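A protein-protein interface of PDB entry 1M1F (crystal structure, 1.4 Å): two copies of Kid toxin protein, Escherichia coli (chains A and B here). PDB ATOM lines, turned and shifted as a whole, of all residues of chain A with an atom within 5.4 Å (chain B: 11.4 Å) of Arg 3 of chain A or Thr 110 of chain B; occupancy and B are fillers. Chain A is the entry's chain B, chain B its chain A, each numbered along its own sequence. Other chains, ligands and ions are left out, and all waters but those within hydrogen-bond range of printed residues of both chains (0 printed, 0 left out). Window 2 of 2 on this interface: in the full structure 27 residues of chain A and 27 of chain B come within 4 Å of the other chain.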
ATOM      1  N   MET A   1     -40.264 -27.503  -4.135  1.00  0.00           N
ATOM      2  CA  MET A   1     -39.453 -26.673  -5.077  1.00  0.00           C
ATOM      3  C   MET A   1     -38.446 -27.667  -5.674  1.00  0.00           C
ATOM      4  O   MET A   1     -37.541 -28.134  -5.000  1.00  0.00           O
ATOM      5  CB  MET A   1     -38.912 -25.452  -4.281  1.00  0.00           C
ATOM      6  CG  MET A   1     -37.815 -24.527  -4.780  1.00  0.00           C
ATOM      7  SD  MET A   1     -38.189 -22.842  -4.047  1.00  0.00           S
ATOM      8  CE  MET A   1     -37.619 -23.013  -2.505  1.00  0.00           C
ATOM      9  N   GLU A   2     -38.727 -28.103  -6.905  1.00  0.00           N
ATOM     10  CA  GLU A   2     -37.930 -29.100  -7.624  1.00  0.00           C
ATOM     11  C   GLU A   2     -36.940 -28.556  -8.663  1.00  0.00           C
ATOM     12  O   GLU A   2     -37.180 -27.525  -9.297  1.00  0.00           O
ATOM     13  CB  GLU A   2     -38.876 -30.042  -8.379  1.00  0.00           C
ATOM     14  CG  GLU A   2     -39.909 -30.792  -7.543  1.00  0.00           C
ATOM     15  CD  GLU A   2     -39.395 -32.094  -6.949  1.00  0.00           C
ATOM     16  OE1 GLU A   2     -38.375 -32.638  -7.429  1.00  0.00           O
ATOM     17  OE2 GLU A   2     -40.033 -32.596  -6.000  1.00  0.00           O
ATOM     18  N   ARG A   3     -35.836 -29.279  -8.833  1.00  0.00           N
ATOM     19  CA  ARG A   3     -34.918 -29.046  -9.935  1.00  0.00           C
ATOM     20  C   ARG A   3     -35.717 -29.082 -11.228  1.00  0.00           C
ATOM     21  O   ARG A   3     -36.529 -29.988 -11.448  1.00  0.00           O
ATOM     22  CB  ARG A   3     -33.856 -30.142  -9.975  1.00  0.00           C
ATOM     23  CG  ARG A   3     -33.021 -30.147 -11.247  1.00  0.00           C
ATOM     24  CD  ARG A   3     -31.975 -31.242 -11.267  1.00  0.00           C
ATOM     25  NE  ARG A   3     -30.832 -30.840 -10.457  1.00  0.00           N
ATOM     26  CZ  ARG A   3     -29.774 -31.592 -10.200  1.00  0.00           C
ATOM     27  NH1 ARG A   3     -28.805 -31.096  -9.441  1.00  0.00           N
ATOM     28  NH2 ARG A   3     -29.681 -32.829 -10.684  1.00  0.00           N
ATOM     29  N   GLY A   4     -35.482 -28.104 -12.092  1.00  0.00           N
ATOM     30  CA  GLY A   4     -36.161 -28.037 -13.370  1.00  0.00           C
ATOM     31  C   GLY A   4     -37.347 -27.101 -13.429  1.00  0.00           C
ATOM     32  O   GLY A   4     -37.902 -26.863 -14.509  1.00  0.00           O
ATOM     33  N   GLU A   5     -37.743 -26.550 -12.293  1.00  0.00           N
ATOM     34  CA  GLU A   5     -38.812 -25.569 -12.286  1.00  0.00           C
ATOM     35  C   GLU A   5     -38.323 -24.174 -12.633  1.00  0.00           C
ATOM     36  O   GLU A   5     -37.240 -23.757 -12.208  1.00  0.00           O
ATOM     37  CB  GLU A   5     -39.487 -25.520 -10.914  1.00  0.00           C
ATOM     38  CG  GLU A   5     -40.279 -26.767 -10.569  1.00  0.00           C
ATOM     39  CD  GLU A   5     -40.817 -26.787  -9.148  1.00  0.00           C
ATOM     40  OE1 GLU A   5     -40.474 -25.911  -8.343  1.00  0.00           O
ATOM     41  OE2 GLU A   5     -41.597 -27.713  -8.827  1.00  0.00           O
ATOM     42  N   ILE A  27     -34.510 -23.501 -11.363  1.00  0.00           N
ATOM     43  CA  ILE A  27     -33.946 -24.139 -10.170  1.00  0.00           C
ATOM     44  C   ILE A  27     -33.032 -25.293 -10.567  1.00  0.00           C
ATOM     45  O   ILE A  27     -33.415 -26.178 -11.336  1.00  0.00           O
ATOM     46  CB  ILE A  27     -35.066 -24.630  -9.233  1.00  0.00           C
ATOM     47  CG1 ILE A  27     -35.883 -23.425  -8.741  1.00  0.00           C
ATOM     48  CG2 ILE A  27     -34.472 -25.413  -8.069  1.00  0.00           C
ATOM     49  CD1 ILE A  27     -36.925 -23.761  -7.718  1.00  0.00           C
ATOM     50  N   VAL A  28     -31.817 -25.251 -10.032  1.00  0.00           N
ATOM     51  CA  VAL A  28     -30.797 -26.246 -10.315  1.00  0.00           C
ATOM     52  C   VAL A  28     -30.664 -27.320  -9.245  1.00  0.00           C
ATOM     53  O   VAL A  28     -30.277 -28.449  -9.541  1.00  0.00           O
ATOM     54  CB  VAL A  28     -29.445 -25.538 -10.451  1.00  0.00           C
ATOM     55  CG1 VAL A  28     -28.269 -26.523 -10.392  1.00  0.00           C
ATOM     56  CG2 VAL A  28     -29.453 -24.703 -11.709  1.00  0.00           C
ATOM     57  N   THR A  29     -30.948 -26.979  -7.998  1.00  0.00           N
ATOM     58  CA  THR A  29     -30.766 -27.920  -6.896  1.00  0.00           C
ATOM     59  C   THR A  29     -32.002 -28.766  -6.641  1.00  0.00           C
ATOM     60  O   THR A  29     -33.117 -28.349  -6.926  1.00  0.00           O
ATOM     61  CB  THR A  29     -30.380 -27.175  -5.618  1.00  0.00           C
ATOM     62  OG1 THR A  29     -31.111 -25.939  -5.535  1.00  0.00           O
ATOM     63  CG2 THR A  29     -28.919 -26.760  -5.654  1.00  0.00           C
ATOM     64  N   PRO A  30     -31.816 -29.960  -6.087  1.00  0.00           N
ATOM     65  CA  PRO A  30     -32.951 -30.856  -5.848  1.00  0.00           C
ATOM     66  C   PRO A  30     -33.851 -30.457  -4.684  1.00  0.00           C
ATOM     67  O   PRO A  30     -33.475 -29.676  -3.804  1.00  0.00           O
ATOM     68  CB  PRO A  30     -32.297 -32.208  -5.550  1.00  0.00           C
ATOM     69  CG  PRO A  30     -30.869 -32.028  -5.641  1.00  0.00           C
ATOM     70  CD  PRO A  30     -30.533 -30.572  -5.706  1.00  0.00           C
ATOM     71  N   ALA A  31     -35.053 -31.032  -4.682  1.00  0.00           N
ATOM     72  CA  ALA A  31     -36.077 -30.729  -3.696  1.00  0.00           C
ATOM     73  C   ALA A  31     -35.624 -30.837  -2.242  1.00  0.00           C
ATOM     74  O   ALA A  31     -35.953 -29.982  -1.442  1.00  0.00           O
ATOM     75  CB  ALA A  31     -37.286 -31.628  -3.909  1.00  0.00           C
ATOM     76  N   ASN A  34     -33.433 -28.034  -1.404  1.00  0.00           N
ATOM     77  CA  ASN A  34     -34.181 -26.788  -1.362  1.00  0.00           C
ATOM     78  C   ASN A  34     -35.002 -26.642  -0.083  1.00  0.00           C
ATOM     79  O   ASN A  34     -35.119 -25.555   0.464  1.00  0.00           O
ATOM     80  CB  ASN A  34     -35.061 -26.665  -2.595  1.00  0.00           C
ATOM     81  CG  ASN A  34     -34.260 -26.657  -3.868  1.00  0.00           C
ATOM     82  OD1 ASN A  34     -33.090 -26.248  -3.875  1.00  0.00           O
ATOM     83  ND2 ASN A  34     -34.872 -27.108  -4.954  1.00  0.00           N
ATOM     84  N   ARG A  92     -42.346 -26.310 -15.550  1.00  0.00           N
ATOM     85  CA  ARG A  92     -41.205 -27.204 -15.418  1.00  0.00           C
ATOM     86  C   ARG A  92     -40.639 -27.499 -16.791  1.00  0.00           C
ATOM     87  O   ARG A  92     -41.403 -27.693 -17.729  1.00  0.00           O
ATOM     88  CB  ARG A  92     -41.648 -28.502 -14.748  1.00  0.00           C
ATOM     89  CG  ARG A  92     -40.539 -29.498 -14.619  1.00  0.00           C
ATOM     90  CD  ARG A  92     -40.649 -30.335 -13.401  1.00  0.00           C
ATOM     91  NE  ARG A  92     -39.544 -31.272 -13.283  1.00  0.00           N
ATOM     92  CZ  ARG A  92     -39.454 -32.168 -12.325  1.00  0.00           C
ATOM     93  NH1 ARG A  92     -40.391 -32.227 -11.388  1.00  0.00           N
ATOM     94  NH2 ARG A  92     -38.435 -33.008 -12.300  1.00  0.00           N
ATOM     95  N   MET A  98     -33.075 -29.761 -18.914  1.00  0.00           N
ATOM     96  CA  MET A  98     -32.373 -29.721 -17.636  1.00  0.00           C
ATOM     97  C   MET A  98     -31.011 -30.394 -17.766  1.00  0.00           C
ATOM     98  O   MET A  98     -30.030 -29.917 -17.209  1.00  0.00           O
ATOM     99  CB  MET A  98     -33.204 -30.377 -16.533  1.00  0.00           C
ATOM    100  CG  MET A  98     -32.702 -30.058 -15.118  1.00  0.00           C
ATOM    101  SD  MET A  98     -32.851 -28.261 -14.698  1.00  0.00           S
ATOM    102  CE  MET A  98     -31.247 -27.925 -14.066  1.00  0.00           C
ATOM    103  N   LEU A 102     -27.480 -28.646 -16.868  1.00  0.00           N
ATOM    104  CA  LEU A 102     -26.520 -29.229 -15.925  1.00  0.00           C
ATOM    105  C   LEU A 102     -25.193 -29.499 -16.617  1.00  0.00           C
ATOM    106  O   LEU A 102     -24.127 -29.327 -16.026  1.00  0.00           O
ATOM    107  CB  LEU A 102     -27.079 -30.514 -15.325  1.00  0.00           C
ATOM    108  CG  LEU A 102     -28.274 -30.311 -14.394  1.00  0.00           C
ATOM    109  CD1 LEU A 102     -28.885 -31.660 -14.069  1.00  0.00           C
ATOM    110  CD2 LEU A 102     -27.899 -29.561 -13.117  1.00  0.00           C
ATOM    111  N   SER A 106     -22.102 -27.577 -15.081  1.00  0.00           N
ATOM    112  CA  SER A 106     -21.096 -28.442 -14.478  1.00  0.00           C
ATOM    113  C   SER A 106     -19.676 -28.044 -14.848  1.00  0.00           C
ATOM    114  O   SER A 106     -18.743 -28.280 -14.070  1.00  0.00           O
ATOM    115  CB  SER A 106     -21.320 -29.923 -14.850  1.00  0.00           C
ATOM    116  OG  SER A 106     -20.997 -30.218 -16.204  1.00  0.00           O
ATOM    117  N   LEU A 109     -16.871 -26.204 -12.786  1.00  0.00           N
ATOM    118  CA  LEU A 109     -16.096 -26.976 -11.804  1.00  0.00           C
ATOM    119  C   LEU A 109     -14.922 -27.725 -12.414  1.00  0.00           C
ATOM    120  O   LEU A 109     -14.160 -28.391 -11.701  1.00  0.00           O
ATOM    121  CB  LEU A 109     -16.988 -28.000 -11.098  1.00  0.00           C
ATOM    122  CG  LEU A 109     -18.291 -27.457 -10.509  1.00  0.00           C
ATOM    123  CD1 LEU A 109     -19.093 -28.611  -9.922  1.00  0.00           C
ATOM    124  CD2 LEU A 109     -18.047 -26.391  -9.454  1.00  0.00           C
ATOM    125  N   ARG B   3      -9.181 -19.413  -9.737  1.00  0.00           N
ATOM    126  CA  ARG B   3      -9.857 -20.362  -8.888  1.00  0.00           C
ATOM    127  C   ARG B   3      -8.962 -20.587  -7.673  1.00  0.00           C
ATOM    128  O   ARG B   3      -7.737 -20.700  -7.799  1.00  0.00           O
ATOM    129  CB  ARG B   3     -10.010 -21.684  -9.626  1.00  0.00           C
ATOM    130  CG  ARG B   3     -10.399 -22.838  -8.732  1.00  0.00           C
ATOM    131  CD  ARG B   3     -10.524 -24.145  -9.482  1.00  0.00           C
ATOM    132  NE  ARG B   3     -11.736 -24.154 -10.289  1.00  0.00           N
ATOM    133  CZ  ARG B   3     -11.896 -24.852 -11.395  1.00  0.00           C
ATOM    134  NH1 ARG B   3     -10.919 -25.629 -11.835  1.00  0.00           N
ATOM    135  NH2 ARG B   3     -13.039 -24.772 -12.063  1.00  0.00           N
ATOM    136  N   VAL B  28     -14.573 -20.047  -7.337  1.00  0.00           N
ATOM    137  CA  VAL B  28     -14.807 -21.384  -7.886  1.00  0.00           C
ATOM    138  C   VAL B  28     -14.400 -21.524  -9.351  1.00  0.00           C
ATOM    139  O   VAL B  28     -13.909 -22.570  -9.767  1.00  0.00           O
ATOM    140  CB  VAL B  28     -16.322 -21.725  -7.769  1.00  0.00           C
ATOM    141  CG1 VAL B  28     -16.688 -23.027  -8.477  1.00  0.00           C
ATOM    142  CG2 VAL B  28     -16.734 -21.777  -6.304  1.00  0.00           C
ATOM    143  N   PHE B  57     -21.986 -29.761   3.502  1.00  0.00           N
ATOM    144  CA  PHE B  57     -21.504 -28.736   2.559  1.00  0.00           C
ATOM    145  C   PHE B  57     -20.474 -27.777   3.145  1.00  0.00           C
ATOM    146  O   PHE B  57     -19.918 -26.953   2.421  1.00  0.00           O
ATOM    147  CB  PHE B  57     -22.680 -27.948   1.982  1.00  0.00           C
ATOM    148  CG  PHE B  57     -23.526 -28.747   1.027  1.00  0.00           C
ATOM    149  CD1 PHE B  57     -23.051 -29.108  -0.219  1.00  0.00           C
ATOM    150  CD2 PHE B  57     -24.801 -29.134   1.380  1.00  0.00           C
ATOM    151  CE1 PHE B  57     -23.831 -29.832  -1.088  1.00  0.00           C
ATOM    152  CE2 PHE B  57     -25.579 -29.865   0.510  1.00  0.00           C
ATOM    153  CZ  PHE B  57     -25.094 -30.210  -0.716  1.00  0.00           C
ATOM    154  N   CYS B  74     -20.260 -24.472   0.811  1.00  0.00           N
ATOM    155  CA  CYS B  74     -20.328 -24.906  -0.577  1.00  0.00           C
ATOM    156  C   CYS B  74     -21.745 -24.965  -1.109  1.00  0.00           C
ATOM    157  O   CYS B  74     -21.953 -25.072  -2.316  1.00  0.00           O
ATOM    158  CB  CYS B  74     -19.654 -26.268  -0.747  1.00  0.00           C
ATOM    159  SG  CYS B  74     -17.925 -26.328  -0.244  1.00  0.00           S
ATOM    160  N   PRO B  77     -23.329 -21.068  -3.575  1.00  0.00           N
ATOM    161  CA  PRO B  77     -22.601 -20.396  -4.652  1.00  0.00           C
ATOM    162  C   PRO B  77     -23.346 -19.155  -5.147  1.00  0.00           C
ATOM    163  O   PRO B  77     -24.585 -19.126  -5.166  1.00  0.00           O
ATOM    164  CB  PRO B  77     -22.545 -21.459  -5.739  1.00  0.00           C
ATOM    165  CG  PRO B  77     -23.755 -22.301  -5.483  1.00  0.00           C
ATOM    166  CD  PRO B  77     -23.828 -22.399  -3.994  1.00  0.00           C
ATOM    167  N   VAL B 101     -13.963 -28.583  -2.105  1.00  0.00           N
ATOM    168  CA  VAL B 101     -15.046 -27.653  -2.420  1.00  0.00           C
ATOM    169  C   VAL B 101     -15.694 -28.000  -3.769  1.00  0.00           C
ATOM    170  O   VAL B 101     -16.923 -28.069  -3.887  1.00  0.00           O
ATOM    171  CB  VAL B 101     -14.520 -26.205  -2.377  1.00  0.00           C
ATOM    172  CG1 VAL B 101     -15.517 -25.216  -2.950  1.00  0.00           C
ATOM    173  CG2 VAL B 101     -14.185 -25.838  -0.949  1.00  0.00           C
ATOM    174  N   LEU B 102     -14.876 -28.229  -4.786  1.00  0.00           N
ATOM    175  CA  LEU B 102     -15.391 -28.630  -6.093  1.00  0.00           C
ATOM    176  C   LEU B 102     -16.195 -29.930  -5.988  1.00  0.00           C
ATOM    177  O   LEU B 102     -17.224 -30.081  -6.643  1.00  0.00           O
ATOM    178  CB  LEU B 102     -14.262 -28.772  -7.111  1.00  0.00           C
ATOM    179  CG  LEU B 102     -13.525 -27.492  -7.495  1.00  0.00           C
ATOM    180  CD1 LEU B 102     -12.360 -27.868  -8.386  1.00  0.00           C
ATOM    181  CD2 LEU B 102     -14.425 -26.477  -8.188  1.00  0.00           C
ATOM    182  N   GLY B 103     -15.726 -30.869  -5.172  1.00  0.00           N
ATOM    183  CA  GLY B 103     -16.442 -32.111  -4.952  1.00  0.00           C
ATOM    184  C   GLY B 103     -17.829 -31.884  -4.380  1.00  0.00           C
ATOM    185  O   GLY B 103     -18.791 -32.520  -4.808  1.00  0.00           O
ATOM    186  N   ARG B 104     -17.944 -30.994  -3.399  1.00  0.00           N
ATOM    187  CA  ARG B 104     -19.253 -30.699  -2.814  1.00  0.00           C
ATOM    188  C   ARG B 104     -20.164 -30.060  -3.865  1.00  0.00           C
ATOM    189  O   ARG B 104     -21.318 -30.441  -3.996  1.00  0.00           O
ATOM    190  CB  ARG B 104     -19.158 -29.754  -1.609  1.00  0.00           C
ATOM    191  CG  ARG B 104     -18.525 -30.277  -0.320  1.00  0.00           C
ATOM    192  CD  ARG B 104     -18.637 -31.713  -0.075  1.00  0.00           C
ATOM    193  NE  ARG B 104     -18.639 -32.002   1.356  1.00  0.00           N
ATOM    194  CZ  ARG B 104     -17.695 -32.671   2.002  1.00  0.00           C
ATOM    195  NH1 ARG B 104     -16.608 -33.114   1.373  1.00  0.00           N
ATOM    196  NH2 ARG B 104     -17.843 -32.887   3.300  1.00  0.00           N
ATOM    197  N   LEU B 105     -19.646 -29.105  -4.626  1.00  0.00           N
ATOM    198  CA  LEU B 105     -20.458 -28.437  -5.637  1.00  0.00           C
ATOM    199  C   LEU B 105     -20.903 -29.403  -6.731  1.00  0.00           C
ATOM    200  O   LEU B 105     -22.004 -29.263  -7.290  1.00  0.00           O
ATOM    201  CB  LEU B 105     -19.681 -27.273  -6.249  1.00  0.00           C
ATOM    202  CG  LEU B 105     -19.570 -26.055  -5.322  1.00  0.00           C
ATOM    203  CD1 LEU B 105     -18.444 -25.128  -5.750  1.00  0.00           C
ATOM    204  CD2 LEU B 105     -20.883 -25.286  -5.273  1.00  0.00           C
ATOM    205  N   SER B 106     -20.067 -30.394  -7.026  1.00  0.00           N
ATOM    206  CA  SER B 106     -20.387 -31.382  -8.047  1.00  0.00           C
ATOM    207  C   SER B 106     -21.660 -32.148  -7.708  1.00  0.00           C
ATOM    208  O   SER B 106     -22.396 -32.564  -8.603  1.00  0.00           O
ATOM    209  CB  SER B 106     -19.233 -32.366  -8.241  1.00  0.00           C
ATOM    210  OG  SER B 106     -19.449 -33.131  -9.418  1.00  0.00           O
ATOM    211  N   THR B 107     -21.941 -32.324  -6.424  1.00  0.00           N
ATOM    212  CA  THR B 107     -23.129 -33.070  -6.026  1.00  0.00           C
ATOM    213  C   THR B 107     -24.428 -32.335  -6.273  1.00  0.00           C
ATOM    214  O   THR B 107     -25.479 -32.973  -6.307  1.00  0.00           O
ATOM    215  CB  THR B 107     -23.085 -33.496  -4.532  1.00  0.00           C
ATOM    216  OG1 THR B 107     -23.211 -32.359  -3.658  1.00  0.00           O
ATOM    217  CG2 THR B 107     -21.780 -34.213  -4.178  1.00  0.00           C
ATOM    218  N   ILE B 108     -24.365 -31.016  -6.443  1.00  0.00           N
ATOM    219  CA  ILE B 108     -25.598 -30.233  -6.633  1.00  0.00           C
ATOM    220  C   ILE B 108     -25.691 -29.473  -7.950  1.00  0.00           C
ATOM    221  O   ILE B 108     -26.789 -29.108  -8.363  1.00  0.00           O
ATOM    222  CB  ILE B 108     -25.846 -29.244  -5.451  1.00  0.00           C
ATOM    223  CG1 ILE B 108     -24.622 -28.366  -5.166  1.00  0.00           C
ATOM    224  CG2 ILE B 108     -26.299 -29.994  -4.220  1.00  0.00           C
ATOM    225  CD1 ILE B 108     -24.935 -27.192  -4.284  1.00  0.00           C
ATOM    226  N   LEU B 109     -24.558 -29.150  -8.566  1.00  0.00           N
ATOM    227  CA  LEU B 109     -24.551 -28.399  -9.825  1.00  0.00           C
ATOM    228  C   LEU B 109     -24.317 -29.245 -11.085  1.00  0.00           C
ATOM    229  O   LEU B 109     -23.915 -28.704 -12.126  1.00  0.00           O
ATOM    230  CB  LEU B 109     -23.487 -27.308  -9.747  1.00  0.00           C
ATOM    231  CG  LEU B 109     -23.595 -26.338  -8.573  1.00  0.00           C
ATOM    232  CD1 LEU B 109     -22.549 -25.275  -8.764  1.00  0.00           C
ATOM    233  CD2 LEU B 109     -24.981 -25.716  -8.401  1.00  0.00           C
ATOM    234  N   THR B 110     -24.604 -30.544 -11.018  1.00  0.00           N
ATOM    235  CA  THR B 110     -24.332 -31.451 -12.137  1.00  0.00           C
ATOM    236  C   THR B 110     -25.291 -32.632 -12.147  1.00  0.00           C
ATOM    237  O   THR B 110     -26.146 -32.809 -11.281  1.00  0.00           O
ATOM    238  CB  THR B 110     -22.860 -32.005 -12.099  1.00  0.00           C
ATOM    239  OG1 THR B 110     -22.753 -33.117 -11.193  1.00  0.00           O
ATOM    240  CG2 THR B 110     -21.862 -30.992 -11.547  1.00  0.00           C
ATOM    241  OXT THR B 110     -25.192 -33.477 -13.044  1.00  0.00           O
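O of Ile 108 of chain B is in hydrogen-bond range of NH1 of Arg 3 of chain A (3.0 Å). The chain-end carboxylate (O) of Thr 110 of chain B lies within salt-bridge range of the guanidinium group (NH2) of Arg 3 of chain A, at 3.6 Å.
The backbone carbonyl oxygen (O) of Val 28 of chain B lies within hydrogen-bond range of the guanidinium group (NE) of Arg 3 of chain B, at 2.7 Å. OG1 of Thr 110 of chain B is in hydrogen-bond range of O of Ser 106 of chain B (2.7 Å). The guanidinium group of Arg 3 of chain A is in hydrogen-bond range of the backbone carbonyl oxygen of Val 28 of chain A, 2.6 Å away. The backbone NH (N) of Arg 3 of chain A lies within hydrogen-bond range of the backbone carbonyl oxygen (O) of Thr 29 of chain A. The side-chain hydroxyl of Thr 29 of chain A lies within hydrogen-bond range of the side-chain amide oxygen of Asn 34 of chain A (2.6 Å). The backbone carbonyl oxygen (O) of Leu 102 of chain A lies close to the side-chain hydroxyl (OG) of Ser 106 of chain A.
Among the printed residues, pairs that only touch across the chains: Ser 106 of chain A with Thr 110 of chain B, Leu 109 of chain A with Arg 3 of chain B, Leu 109 of chain A with Ser 106 of chain B, Val 28 of chain A with Ile 108 of chain B, Ser 106 of chain A with Leu 109 of chain B, Leu 109 of chain A with Leu 105 of chain B, Leu 109 of chain A with Val 28 of chain B, Leu 109 of chain A with Leu 102 of chain B, Val 28 of chain A with Leu 109 of chain B, Leu 102 of chain A with Leu 109 of chain B, Thr 29 of chain A with Ile 108 of chain B and Leu 109 of chain A with Thr 110 of chain B.
No residue of chain B comes within 4 Å of Glu 2 of chain A. Arg 3 of chain A touches just these residues of chain B: Ile 108 (3.0 Å) and Thr 110 (3.6 Å). No residue of chain B comes within 4 Å of Gly 4 of chain A. No residue of chain B comes within 4 Å of Glu 5 of chain A. Val 28 of chain A touches just these residues of chain B: Ile 108 and Leu 109. Of the printed residues of chain B, Thr 29 of chain A touches Ile 108 (3.96 Å). No residue of chain B comes within 4 Å of Pro 30 of chain A. Ala 31 of chain A touches none of the printed residues of chain B. Of the printed residues of chain B, Leu 102 of chain A touches Leu 109 (3.96 Å). Ser 106 of chain A touches just these residues of chain B: Leu 109 (3.6 Å) and Thr 110 (3.5 Å). Printed residues of chain A within 4 Å of Leu 105 of chain B: Leu 109. Of the printed residues of chain A, Ser 106 of chain B touches Leu 109 (3.5 Å). Printed residues of chain A within 4 Å of Thr 110 of chain B: Arg 3 (3.6 Å), Ser 106 (3.5 Å) and Leu 109 (3.997 Å). The nearest printed residue of chain A that does not touch Thr 110 of chain B is Leu 102 of chain A (4.03 Å). The nearest printed residue of chain A that does not touch Ser 106 of chain B is Ser 106 of chain A (6.6 Å).
Printed residues of chain A that touch a printed residue of chain B: Arg 3, Val 28, Thr 29, Leu 102, Ser 106 and Leu 109. Hydrophobic or aromatic side chains of chain A within 4 Å of the printed part of chain B: Val 28 and Leu 109. Among the printed residues, no Asp or Glu carboxylate lies within 4 Å of a Lys or Arg side-chain nitrogen of the other chain.
Val 28 of chain A touches Leu 109 of chain B, and with the chains exchanged Leu 109 of chain A touches Val 28 of chain B. Leu 102 of chain A touches Leu 109 of chain B, and with the chains exchanged Leu 109 of chain A touches Leu 102 of chain B. Ser 106 of chain A touches Leu 109 of chain B, and with the chains exchanged Leu 109 of chain A touches Ser 106 of chain B. Leu 109 of chain A touches Arg 3 of chain B, but with the chains exchanged Arg 3 of chain A does not touch Leu 109 of chain B (4.8 Å). Of the 14 pairs that touch across the chains among the printed residues, 6 have their exchanged pair printed and touching as well.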
